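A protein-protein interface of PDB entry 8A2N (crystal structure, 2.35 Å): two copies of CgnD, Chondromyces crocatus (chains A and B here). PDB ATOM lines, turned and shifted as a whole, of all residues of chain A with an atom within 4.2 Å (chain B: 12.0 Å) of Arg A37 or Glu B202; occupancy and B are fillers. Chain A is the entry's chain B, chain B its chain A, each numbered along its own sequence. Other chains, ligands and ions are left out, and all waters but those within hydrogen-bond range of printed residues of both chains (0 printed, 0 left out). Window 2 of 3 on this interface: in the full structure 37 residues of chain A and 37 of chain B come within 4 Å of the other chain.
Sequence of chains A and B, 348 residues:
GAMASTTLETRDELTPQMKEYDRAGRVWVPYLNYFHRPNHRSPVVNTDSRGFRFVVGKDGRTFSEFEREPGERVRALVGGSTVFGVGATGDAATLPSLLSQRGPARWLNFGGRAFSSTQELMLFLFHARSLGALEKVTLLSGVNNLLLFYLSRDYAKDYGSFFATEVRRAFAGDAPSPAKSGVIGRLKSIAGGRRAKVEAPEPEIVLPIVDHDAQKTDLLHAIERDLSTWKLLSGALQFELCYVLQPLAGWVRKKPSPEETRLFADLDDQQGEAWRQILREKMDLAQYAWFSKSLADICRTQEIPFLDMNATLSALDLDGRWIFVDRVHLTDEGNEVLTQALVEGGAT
NH1 of Arg A37 is in hydrogen-bond range of O of Pro B203, 2.6 Å away.
The side-chain carboxylate (OE2) of Glu B204 is in salt-bridge range of the guanidinium group (NH1) of Arg A37 (3.3 Å).
NH1 of Arg A37 lies close to N of Glu B202 (3.3 Å).
No position is printed for both chains.
Of chain B, only Glu B202, Pro B203 and Glu B204 come within 4 Å of Arg A37.
Glu B202 touches one residue of chain A.
No residue of chain B comes within 4 Å of Ala A24.
Printed residues of chain B within 4 Å of Val A27: Pro B203 (3.6 Å), Glu B204 (3.9 Å) and Ile B205 (3.9 Å).
Phe A35 touches none of the printed residues of chain B.
Of chain B, only Ile B205 comes within 4 Å of His A36.
No residue of chain B comes within 4 Å of Asn A39.
No residue of chain B comes within 4 Å of His A40.
Of the printed residues of chain A, Glu B204 touches Val A27, Arg A37 and Pro A38.
Of the printed residues of chain A, Pro B203 touches Val A27 (3.6 Å), Arg A37 (2.6 Å) and Pro A38 (3.7 Å).
Asp B158 touches none of the printed residues of chain A.
Asp B154 touches none of the printed residues of chain A.
The nearest printed residue of chain A that does not touch Glu B202 is Val A27 (6.4 Å).
The nearest printed residue of chain A that does not touch Ile B205 is Phe A35 (4.2 Å).
Among the printed residues, pairs that only touch across the chains: Val A27 with Pro B203, Pro A38 with Glu B204, Pro A38 with Pro B203, His A36 with Ile B205, Val A27 with Glu B204, Val A27 with Ile B205 and Pro A38 with Ile B205.
Of the 11 printed residues of chain A, 4 touch a printed residue of chain B.
Printed residues of chain A that touch a printed residue of chain B: Val A27, His A36, Arg A37 and Pro A38.
Printed residues of chain B that touch a printed residue of chain A: Glu B202, Pro B203, Glu B204 and Ile B205.
Hydrophobic or aromatic side chains of chain B within 4 Å of the printed part of chain A: Pro B203 and Ile B205.
The backbone carbonyl oxygen of Gly A25 sits at hydrogen-bond distance from the backbone NH of Arg A37 (3.2 Å).
The backbone carbonyl oxygen (O) of Arg A26 is in hydrogen-bond range of the guanidinium group (NH2) of Arg A37.
N of Val A27 is in hydrogen-bond range of O of Phe A35 (3.0 Å).
The side-chain hydroxyl of Thr A47 is in hydrogen-bond range of the backbone carbonyl oxygen of Arg A37.
OE1 of Glu B204 lies within salt-bridge range of NH2 of Arg B168 (2.9 Å).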
ATOM      1  N   ALA A  24      10.923  16.685 -12.416  1.00  0.00           N
ATOM      2  CA  ALA A  24      10.700  16.611 -13.858  1.00  0.00           C
ATOM      3  C   ALA A  24       9.820  17.756 -14.313  1.00  0.00           C
ATOM      4  O   ALA A  24      10.061  18.356 -15.383  1.00  0.00           O
ATOM      5  CB  ALA A  24      10.077  15.279 -14.240  1.00  0.00           C
ATOM      6  N   GLY A  25       8.805  18.089 -13.515  1.00  0.00           N
ATOM      7  CA  GLY A  25       8.081  19.316 -13.762  1.00  0.00           C
ATOM      8  C   GLY A  25       6.745  19.097 -14.461  1.00  0.00           C
ATOM      9  O   GLY A  25       6.517  18.110 -15.182  1.00  0.00           O
ATOM     10  N   ARG A  26       5.895  20.104 -14.300  1.00  0.00           N
ATOM     11  CA  ARG A  26       4.498  20.109 -14.733  1.00  0.00           C
ATOM     12  C   ARG A  26       4.172  21.555 -15.123  1.00  0.00           C
ATOM     13  O   ARG A  26       4.494  22.490 -14.386  1.00  0.00           O
ATOM     14  CB  ARG A  26       3.602  19.654 -13.580  1.00  0.00           C
ATOM     15  CG  ARG A  26       3.418  18.079 -13.387  1.00  0.00           C
ATOM     16  CD  ARG A  26       2.820  17.892 -11.928  1.00  0.00           C
ATOM     17  NE  ARG A  26       2.080  16.654 -11.622  1.00  0.00           N
ATOM     18  CZ  ARG A  26       2.509  15.621 -10.889  1.00  0.00           C
ATOM     19  NH1 ARG A  26       3.730  15.566 -10.326  1.00  0.00           N
ATOM     20  NH2 ARG A  26       1.646  14.631 -10.694  1.00  0.00           N
ATOM     21  N   VAL A  27       3.570  21.737 -16.287  1.00  0.00           N
ATOM     22  CA  VAL A  27       3.227  23.037 -16.850  1.00  0.00           C
ATOM     23  C   VAL A  27       1.737  23.078 -17.143  1.00  0.00           C
ATOM     24  O   VAL A  27       1.081  22.042 -17.351  1.00  0.00           O
ATOM     25  CB  VAL A  27       4.018  23.340 -18.148  1.00  0.00           C
ATOM     26  CG1 VAL A  27       5.461  23.594 -17.829  1.00  0.00           C
ATOM     27  CG2 VAL A  27       3.871  22.222 -19.140  1.00  0.00           C
ATOM     28  N   PHE A  35       0.266  19.279 -18.276  1.00  0.00           N
ATOM     29  CA  PHE A  35       1.017  18.200 -18.866  1.00  0.00           C
ATOM     30  C   PHE A  35       2.431  18.308 -18.318  1.00  0.00           C
ATOM     31  O   PHE A  35       2.713  19.131 -17.453  1.00  0.00           O
ATOM     32  CB  PHE A  35       0.935  18.265 -20.399  1.00  0.00           C
ATOM     33  CG  PHE A  35       1.260  16.956 -21.074  1.00  0.00           C
ATOM     34  CD1 PHE A  35       0.734  15.771 -20.618  1.00  0.00           C
ATOM     35  CD2 PHE A  35       2.120  16.920 -22.140  1.00  0.00           C
ATOM     36  CE1 PHE A  35       1.063  14.579 -21.208  1.00  0.00           C
ATOM     37  CE2 PHE A  35       2.452  15.721 -22.744  1.00  0.00           C
ATOM     38  CZ  PHE A  35       1.916  14.564 -22.297  1.00  0.00           C
ATOM     39  N   HIS A  36       3.324  17.464 -18.811  1.00  0.00           N
ATOM     40  CA  HIS A  36       4.715  17.453 -18.352  1.00  0.00           C
ATOM     41  C   HIS A  36       5.519  18.584 -18.974  1.00  0.00           C
ATOM     42  O   HIS A  36       5.276  18.993 -20.098  1.00  0.00           O
ATOM     43  CB  HIS A  36       5.374  16.128 -18.697  1.00  0.00           C
ATOM     44  CG  HIS A  36       4.456  14.969 -18.550  1.00  0.00           C
ATOM     45  ND1 HIS A  36       4.065  14.202 -19.619  1.00  0.00           N
ATOM     46  CD2 HIS A  36       3.798  14.479 -17.474  1.00  0.00           C
ATOM     47  CE1 HIS A  36       3.236  13.258 -19.208  1.00  0.00           C
ATOM     48  NE2 HIS A  36       3.030  13.422 -17.916  1.00  0.00           N
ATOM     49  N   ARG A  37       6.455  19.109 -18.211  1.00  0.00           N
ATOM     50  CA  ARG A  37       7.383  20.099 -18.728  1.00  0.00           C
ATOM     51  C   ARG A  37       8.136  19.493 -19.909  1.00  0.00           C
ATOM     52  O   ARG A  37       8.572  18.332 -19.830  1.00  0.00           O
ATOM     53  CB  ARG A  37       8.340  20.525 -17.617  1.00  0.00           C
ATOM     54  CG  ARG A  37       9.363  21.561 -18.013  1.00  0.00           C
ATOM     55  CD  ARG A  37       9.987  22.267 -16.771  1.00  0.00           C
ATOM     56  NE  ARG A  37       8.965  22.665 -15.789  1.00  0.00           N
ATOM     57  CZ  ARG A  37       8.421  23.887 -15.713  1.00  0.00           C
ATOM     58  NH1 ARG A  37       8.800  24.880 -16.544  1.00  0.00           N
ATOM     59  NH2 ARG A  37       7.494  24.124 -14.793  1.00  0.00           N
ATOM     60  N   PRO A  38       8.238  20.190 -21.036  1.00  0.00           N
ATOM     61  CA  PRO A  38       8.880  19.607 -22.210  1.00  0.00           C
ATOM     62  C   PRO A  38      10.401  19.728 -22.172  1.00  0.00           C
ATOM     63  O   PRO A  38      10.988  20.585 -21.503  1.00  0.00           O
ATOM     64  CB  PRO A  38       8.303  20.431 -23.369  1.00  0.00           C
ATOM     65  CG  PRO A  38       8.035  21.759 -22.773  1.00  0.00           C
ATOM     66  CD  PRO A  38       7.603  21.481 -21.347  1.00  0.00           C
ATOM     67  N   ASN A  39      11.040  18.845 -22.947  1.00  0.00           N
ATOM     68  CA  ASN A  39      12.510  18.862 -23.135  1.00  0.00           C
ATOM     69  C   ASN A  39      13.285  18.635 -21.834  1.00  0.00           C
ATOM     70  O   ASN A  39      14.418  19.082 -21.688  1.00  0.00           O
ATOM     71  CB  ASN A  39      12.931  20.178 -23.796  1.00  0.00           C
ATOM     72  CG  ASN A  39      12.221  20.369 -25.120  1.00  0.00           C
ATOM     73  OD1 ASN A  39      12.220  19.447 -25.964  1.00  0.00           O
ATOM     74  ND2 ASN A  39      11.578  21.518 -25.304  1.00  0.00           N
ATOM     75  N   HIS A  40      12.664  17.934 -20.870  1.00  0.00           N
ATOM     76  CA  HIS A  40      13.352  17.635 -19.630  1.00  0.00           C
ATOM     77  C   HIS A  40      14.414  16.566 -19.883  1.00  0.00           C
ATOM     78  O   HIS A  40      14.183  15.601 -20.623  1.00  0.00           O
ATOM     79  CB  HIS A  40      12.364  17.167 -18.574  1.00  0.00           C
ATOM     80  CG  HIS A  40      12.998  16.919 -17.241  1.00  0.00           C
ATOM     81  ND1 HIS A  40      13.298  17.932 -16.363  1.00  0.00           N
ATOM     82  CD2 HIS A  40      13.424  15.779 -16.658  1.00  0.00           C
ATOM     83  CE1 HIS A  40      13.857  17.427 -15.282  1.00  0.00           C
ATOM     84  NE2 HIS A  40      13.942  16.125 -15.437  1.00  0.00           N
ATOM     85  N   THR A  47      11.656  13.973 -21.531  1.00  0.00           N
ATOM     86  CA  THR A  47      10.470  14.294 -22.307  1.00  0.00           C
ATOM     87  C   THR A  47      10.849  15.072 -23.564  1.00  0.00           C
ATOM     88  O   THR A  47      11.816  15.825 -23.582  1.00  0.00           O
ATOM     89  CB  THR A  47       9.511  15.117 -21.481  1.00  0.00           C
ATOM     90  OG1 THR A  47      10.196  16.272 -20.991  1.00  0.00           O
ATOM     91  CG2 THR A  47       8.964  14.307 -20.336  1.00  0.00           C
ATOM     92  N   ASP B 154       0.183  34.640 -24.909  1.00  0.00           N
ATOM     93  CA  ASP B 154       0.851  33.352 -24.963  1.00  0.00           C
ATOM     94  C   ASP B 154      -0.017  32.398 -25.761  1.00  0.00           C
ATOM     95  O   ASP B 154      -1.231  32.559 -25.839  1.00  0.00           O
ATOM     96  CB  ASP B 154       1.093  32.784 -23.557  1.00  0.00           C
ATOM     97  CG  ASP B 154       2.110  33.591 -22.754  1.00  0.00           C
ATOM     98  OD1 ASP B 154       2.369  34.770 -23.082  1.00  0.00           O
ATOM     99  OD2 ASP B 154       2.681  33.045 -21.770  1.00  0.00           O
ATOM    100  N   TYR B 155       0.610  31.407 -26.370  1.00  0.00           N
ATOM    101  CA  TYR B 155      -0.112  30.533 -27.280  1.00  0.00           C
ATOM    102  C   TYR B 155       0.604  29.184 -27.401  1.00  0.00           C
ATOM    103  O   TYR B 155       1.826  29.128 -27.491  1.00  0.00           O
ATOM    104  CB  TYR B 155      -0.248  31.167 -28.656  1.00  0.00           C
ATOM    105  CG  TYR B 155      -1.311  30.473 -29.506  1.00  0.00           C
ATOM    106  CD1 TYR B 155      -2.669  30.644 -29.243  1.00  0.00           C
ATOM    107  CD2 TYR B 155      -0.951  29.653 -30.559  1.00  0.00           C
ATOM    108  CE1 TYR B 155      -3.622  30.051 -30.008  1.00  0.00           C
ATOM    109  CE2 TYR B 155      -1.917  29.027 -31.335  1.00  0.00           C
ATOM    110  CZ  TYR B 155      -3.253  29.243 -31.053  1.00  0.00           C
ATOM    111  OH  TYR B 155      -4.221  28.614 -31.809  1.00  0.00           O
ATOM    112  N   ASP B 158      -0.341  23.488 -30.504  1.00  0.00           N
ATOM    113  CA  ASP B 158      -1.024  22.189 -30.565  1.00  0.00           C
ATOM    114  C   ASP B 158      -2.383  22.218 -29.914  1.00  0.00           C
ATOM    115  O   ASP B 158      -3.257  21.463 -30.262  1.00  0.00           O
ATOM    116  CB  ASP B 158      -0.174  21.102 -29.892  1.00  0.00           C
ATOM    117  CG  ASP B 158       1.029  20.722 -30.702  1.00  0.00           C
ATOM    118  OD1 ASP B 158       0.960  20.837 -31.954  1.00  0.00           O
ATOM    119  OD2 ASP B 158       2.046  20.274 -30.096  1.00  0.00           O
ATOM    120  N   TYR B 159      -2.558  23.097 -28.940  1.00  0.00           N
ATOM    121  CA  TYR B 159      -3.779  23.145 -28.154  1.00  0.00           C
ATOM    122  C   TYR B 159      -4.658  24.338 -28.482  1.00  0.00           C
ATOM    123  O   TYR B 159      -5.890  24.214 -28.466  1.00  0.00           O
ATOM    124  CB  TYR B 159      -3.433  23.165 -26.659  1.00  0.00           C
ATOM    125  CG  TYR B 159      -2.597  21.978 -26.297  1.00  0.00           C
ATOM    126  CD1 TYR B 159      -3.145  20.718 -26.253  1.00  0.00           C
ATOM    127  CD2 TYR B 159      -1.247  22.110 -26.051  1.00  0.00           C
ATOM    128  CE1 TYR B 159      -2.386  19.614 -25.950  1.00  0.00           C
ATOM    129  CE2 TYR B 159      -0.461  20.991 -25.717  1.00  0.00           C
ATOM    130  CZ  TYR B 159      -1.043  19.758 -25.688  1.00  0.00           C
ATOM    131  OH  TYR B 159      -0.310  18.650 -25.422  1.00  0.00           O
ATOM    132  N   ARG B 168      -5.075  30.684 -16.507  1.00  0.00           N
ATOM    133  CA  ARG B 168      -3.706  30.260 -16.221  1.00  0.00           C
ATOM    134  C   ARG B 168      -3.097  31.150 -15.132  1.00  0.00           C
ATOM    135  O   ARG B 168      -2.892  32.350 -15.354  1.00  0.00           O
ATOM    136  CB  ARG B 168      -2.839  30.311 -17.482  1.00  0.00           C
ATOM    137  CG  ARG B 168      -1.351  30.494 -17.193  1.00  0.00           C
ATOM    138  CD  ARG B 168      -0.494  30.349 -18.433  1.00  0.00           C
ATOM    139  NE  ARG B 168       0.875  30.013 -18.080  1.00  0.00           N
ATOM    140  CZ  ARG B 168       1.933  30.189 -18.877  1.00  0.00           C
ATOM    141  NH1 ARG B 168       1.776  30.705 -20.097  1.00  0.00           N
ATOM    142  NH2 ARG B 168       3.154  29.849 -18.451  1.00  0.00           N
ATOM    143  N   ARG B 169      -2.793  30.554 -13.977  1.00  0.00           N
ATOM    144  CA  ARG B 169      -2.181  31.262 -12.845  1.00  0.00           C
ATOM    145  C   ARG B 169      -2.155  30.345 -11.598  1.00  0.00           C
ATOM    146  O   ARG B 169      -2.121  29.112 -11.698  1.00  0.00           O
ATOM    147  CB  ARG B 169      -2.920  32.575 -12.516  1.00  0.00           C
ATOM    148  CG  ARG B 169      -4.216  32.394 -11.749  1.00  0.00           C
ATOM    149  CD  ARG B 169      -5.207  31.632 -12.627  1.00  0.00           C
ATOM    150  NE  ARG B 169      -6.510  31.407 -12.005  1.00  0.00           N
ATOM    151  CZ  ARG B 169      -6.783  30.401 -11.181  1.00  0.00           C
ATOM    152  NH1 ARG B 169      -8.007  30.287 -10.677  1.00  0.00           N
ATOM    153  NH2 ARG B 169      -5.841  29.512 -10.856  1.00  0.00           N
ATOM    154  N   GLU B 202      11.683  26.380 -16.275  1.00  0.00           N
ATOM    155  CA  GLU B 202      11.556  27.486 -17.230  1.00  0.00           C
ATOM    156  C   GLU B 202      10.836  27.093 -18.529  1.00  0.00           C
ATOM    157  O   GLU B 202      10.019  27.867 -19.032  1.00  0.00           O
ATOM    158  CB  GLU B 202      12.949  28.063 -17.559  1.00  0.00           C
ATOM    159  CG  GLU B 202      12.927  29.201 -18.584  1.00  0.00           C
ATOM    160  CD  GLU B 202      13.946  30.302 -18.267  1.00  0.00           C
ATOM    161  OE1 GLU B 202      14.643  30.210 -17.217  1.00  0.00           O
ATOM    162  OE2 GLU B 202      14.059  31.258 -19.076  1.00  0.00           O
ATOM    163  N   PRO B 203      11.131  25.914 -19.085  1.00  0.00           N
ATOM    164  CA  PRO B 203      10.490  25.528 -20.355  1.00  0.00           C
ATOM    165  C   PRO B 203       8.983  25.378 -20.184  1.00  0.00           C
ATOM    166  O   PRO B 203       8.502  24.894 -19.164  1.00  0.00           O
ATOM    167  CB  PRO B 203      11.157  24.188 -20.710  1.00  0.00           C
ATOM    168  CG  PRO B 203      12.393  24.122 -19.920  1.00  0.00           C
ATOM    169  CD  PRO B 203      12.161  24.936 -18.668  1.00  0.00           C
ATOM    170  N   GLU B 204       8.243  25.776 -21.209  1.00  0.00           N
ATOM    171  CA  GLU B 204       6.792  25.774 -21.182  1.00  0.00           C
ATOM    172  C   GLU B 204       6.260  25.226 -22.489  1.00  0.00           C
ATOM    173  O   GLU B 204       6.967  25.134 -23.484  1.00  0.00           O
ATOM    174  CB  GLU B 204       6.235  27.200 -20.971  1.00  0.00           C
ATOM    175  CG  GLU B 204       6.782  27.903 -19.732  1.00  0.00           C
ATOM    176  CD  GLU B 204       6.029  27.497 -18.465  1.00  0.00           C
ATOM    177  OE1 GLU B 204       4.779  27.426 -18.526  1.00  0.00           O
ATOM    178  OE2 GLU B 204       6.691  27.242 -17.428  1.00  0.00           O
ATOM    179  N   ILE B 205       4.984  24.869 -22.477  1.00  0.00           N
ATOM    180  CA  ILE B 205       4.297  24.534 -23.719  1.00  0.00           C
ATOM    181  C   ILE B 205       3.605  25.770 -24.311  1.00  0.00           C
ATOM    182  O   ILE B 205       3.655  26.019 -25.520  1.00  0.00           O
ATOM    183  CB  ILE B 205       3.313  23.375 -23.452  1.00  0.00           C
ATOM    184  CG1 ILE B 205       4.089  22.137 -23.035  1.00  0.00           C
ATOM    185  CG2 ILE B 205       2.417  23.125 -24.677  1.00  0.00           C
ATOM    186  CD1 ILE B 205       3.281  20.898 -22.797  1.00  0.00           C
ATOM    187  N   VAL B 206       2.967  26.572 -23.471  1.00  0.00           N
ATOM    188  CA  VAL B 206       2.349  27.817 -23.902  1.00  0.00           C
ATOM    189  C   VAL B 206       3.452  28.871 -23.945  1.00  0.00           C
ATOM    190  O   VAL B 206       3.994  29.257 -22.909  1.00  0.00           O
ATOM    191  CB  VAL B 206       1.206  28.239 -22.961  1.00  0.00           C
ATOM    192  CG1 VAL B 206       0.398  29.349 -23.564  1.00  0.00           C
ATOM    193  CG2 VAL B 206       0.298  27.048 -22.664  1.00  0.00           C
ATOM    194  N   LEU B 207       3.773  29.361 -25.164  1.00  0.00           N
ATOM    195  CA  LEU B 207       4.902  30.275 -25.370  1.00  0.00           C
ATOM    196  C   LEU B 207       4.410  31.696 -25.618  1.00  0.00           C
ATOM    197  O   LEU B 207       3.348  31.908 -26.201  1.00  0.00           O
ATOM    198  CB  LEU B 207       5.751  29.825 -26.570  1.00  0.00           C
ATOM    199  CG  LEU B 207       6.356  28.414 -26.468  1.00  0.00           C
ATOM    200  CD1 LEU B 207       6.962  27.983 -27.796  1.00  0.00           C
ATOM    201  CD2 LEU B 207       7.401  28.399 -25.396  1.00  0.00           C
ATOM    202  N   PRO B 208       5.155  32.690 -25.169  1.00  0.00           N
ATOM    203  CA  PRO B 208       4.819  34.075 -25.528  1.00  0.00           C
ATOM    204  C   PRO B 208       4.928  34.334 -27.020  1.00  0.00           C
ATOM    205  O   PRO B 208       5.868  33.895 -27.680  1.00  0.00           O
ATOM    206  CB  PRO B 208       5.847  34.907 -24.739  1.00  0.00           C
ATOM    207  CG  PRO B 208       6.962  33.976 -24.455  1.00  0.00           C
ATOM    208  CD  PRO B 208       6.339  32.624 -24.285  1.00  0.00           C
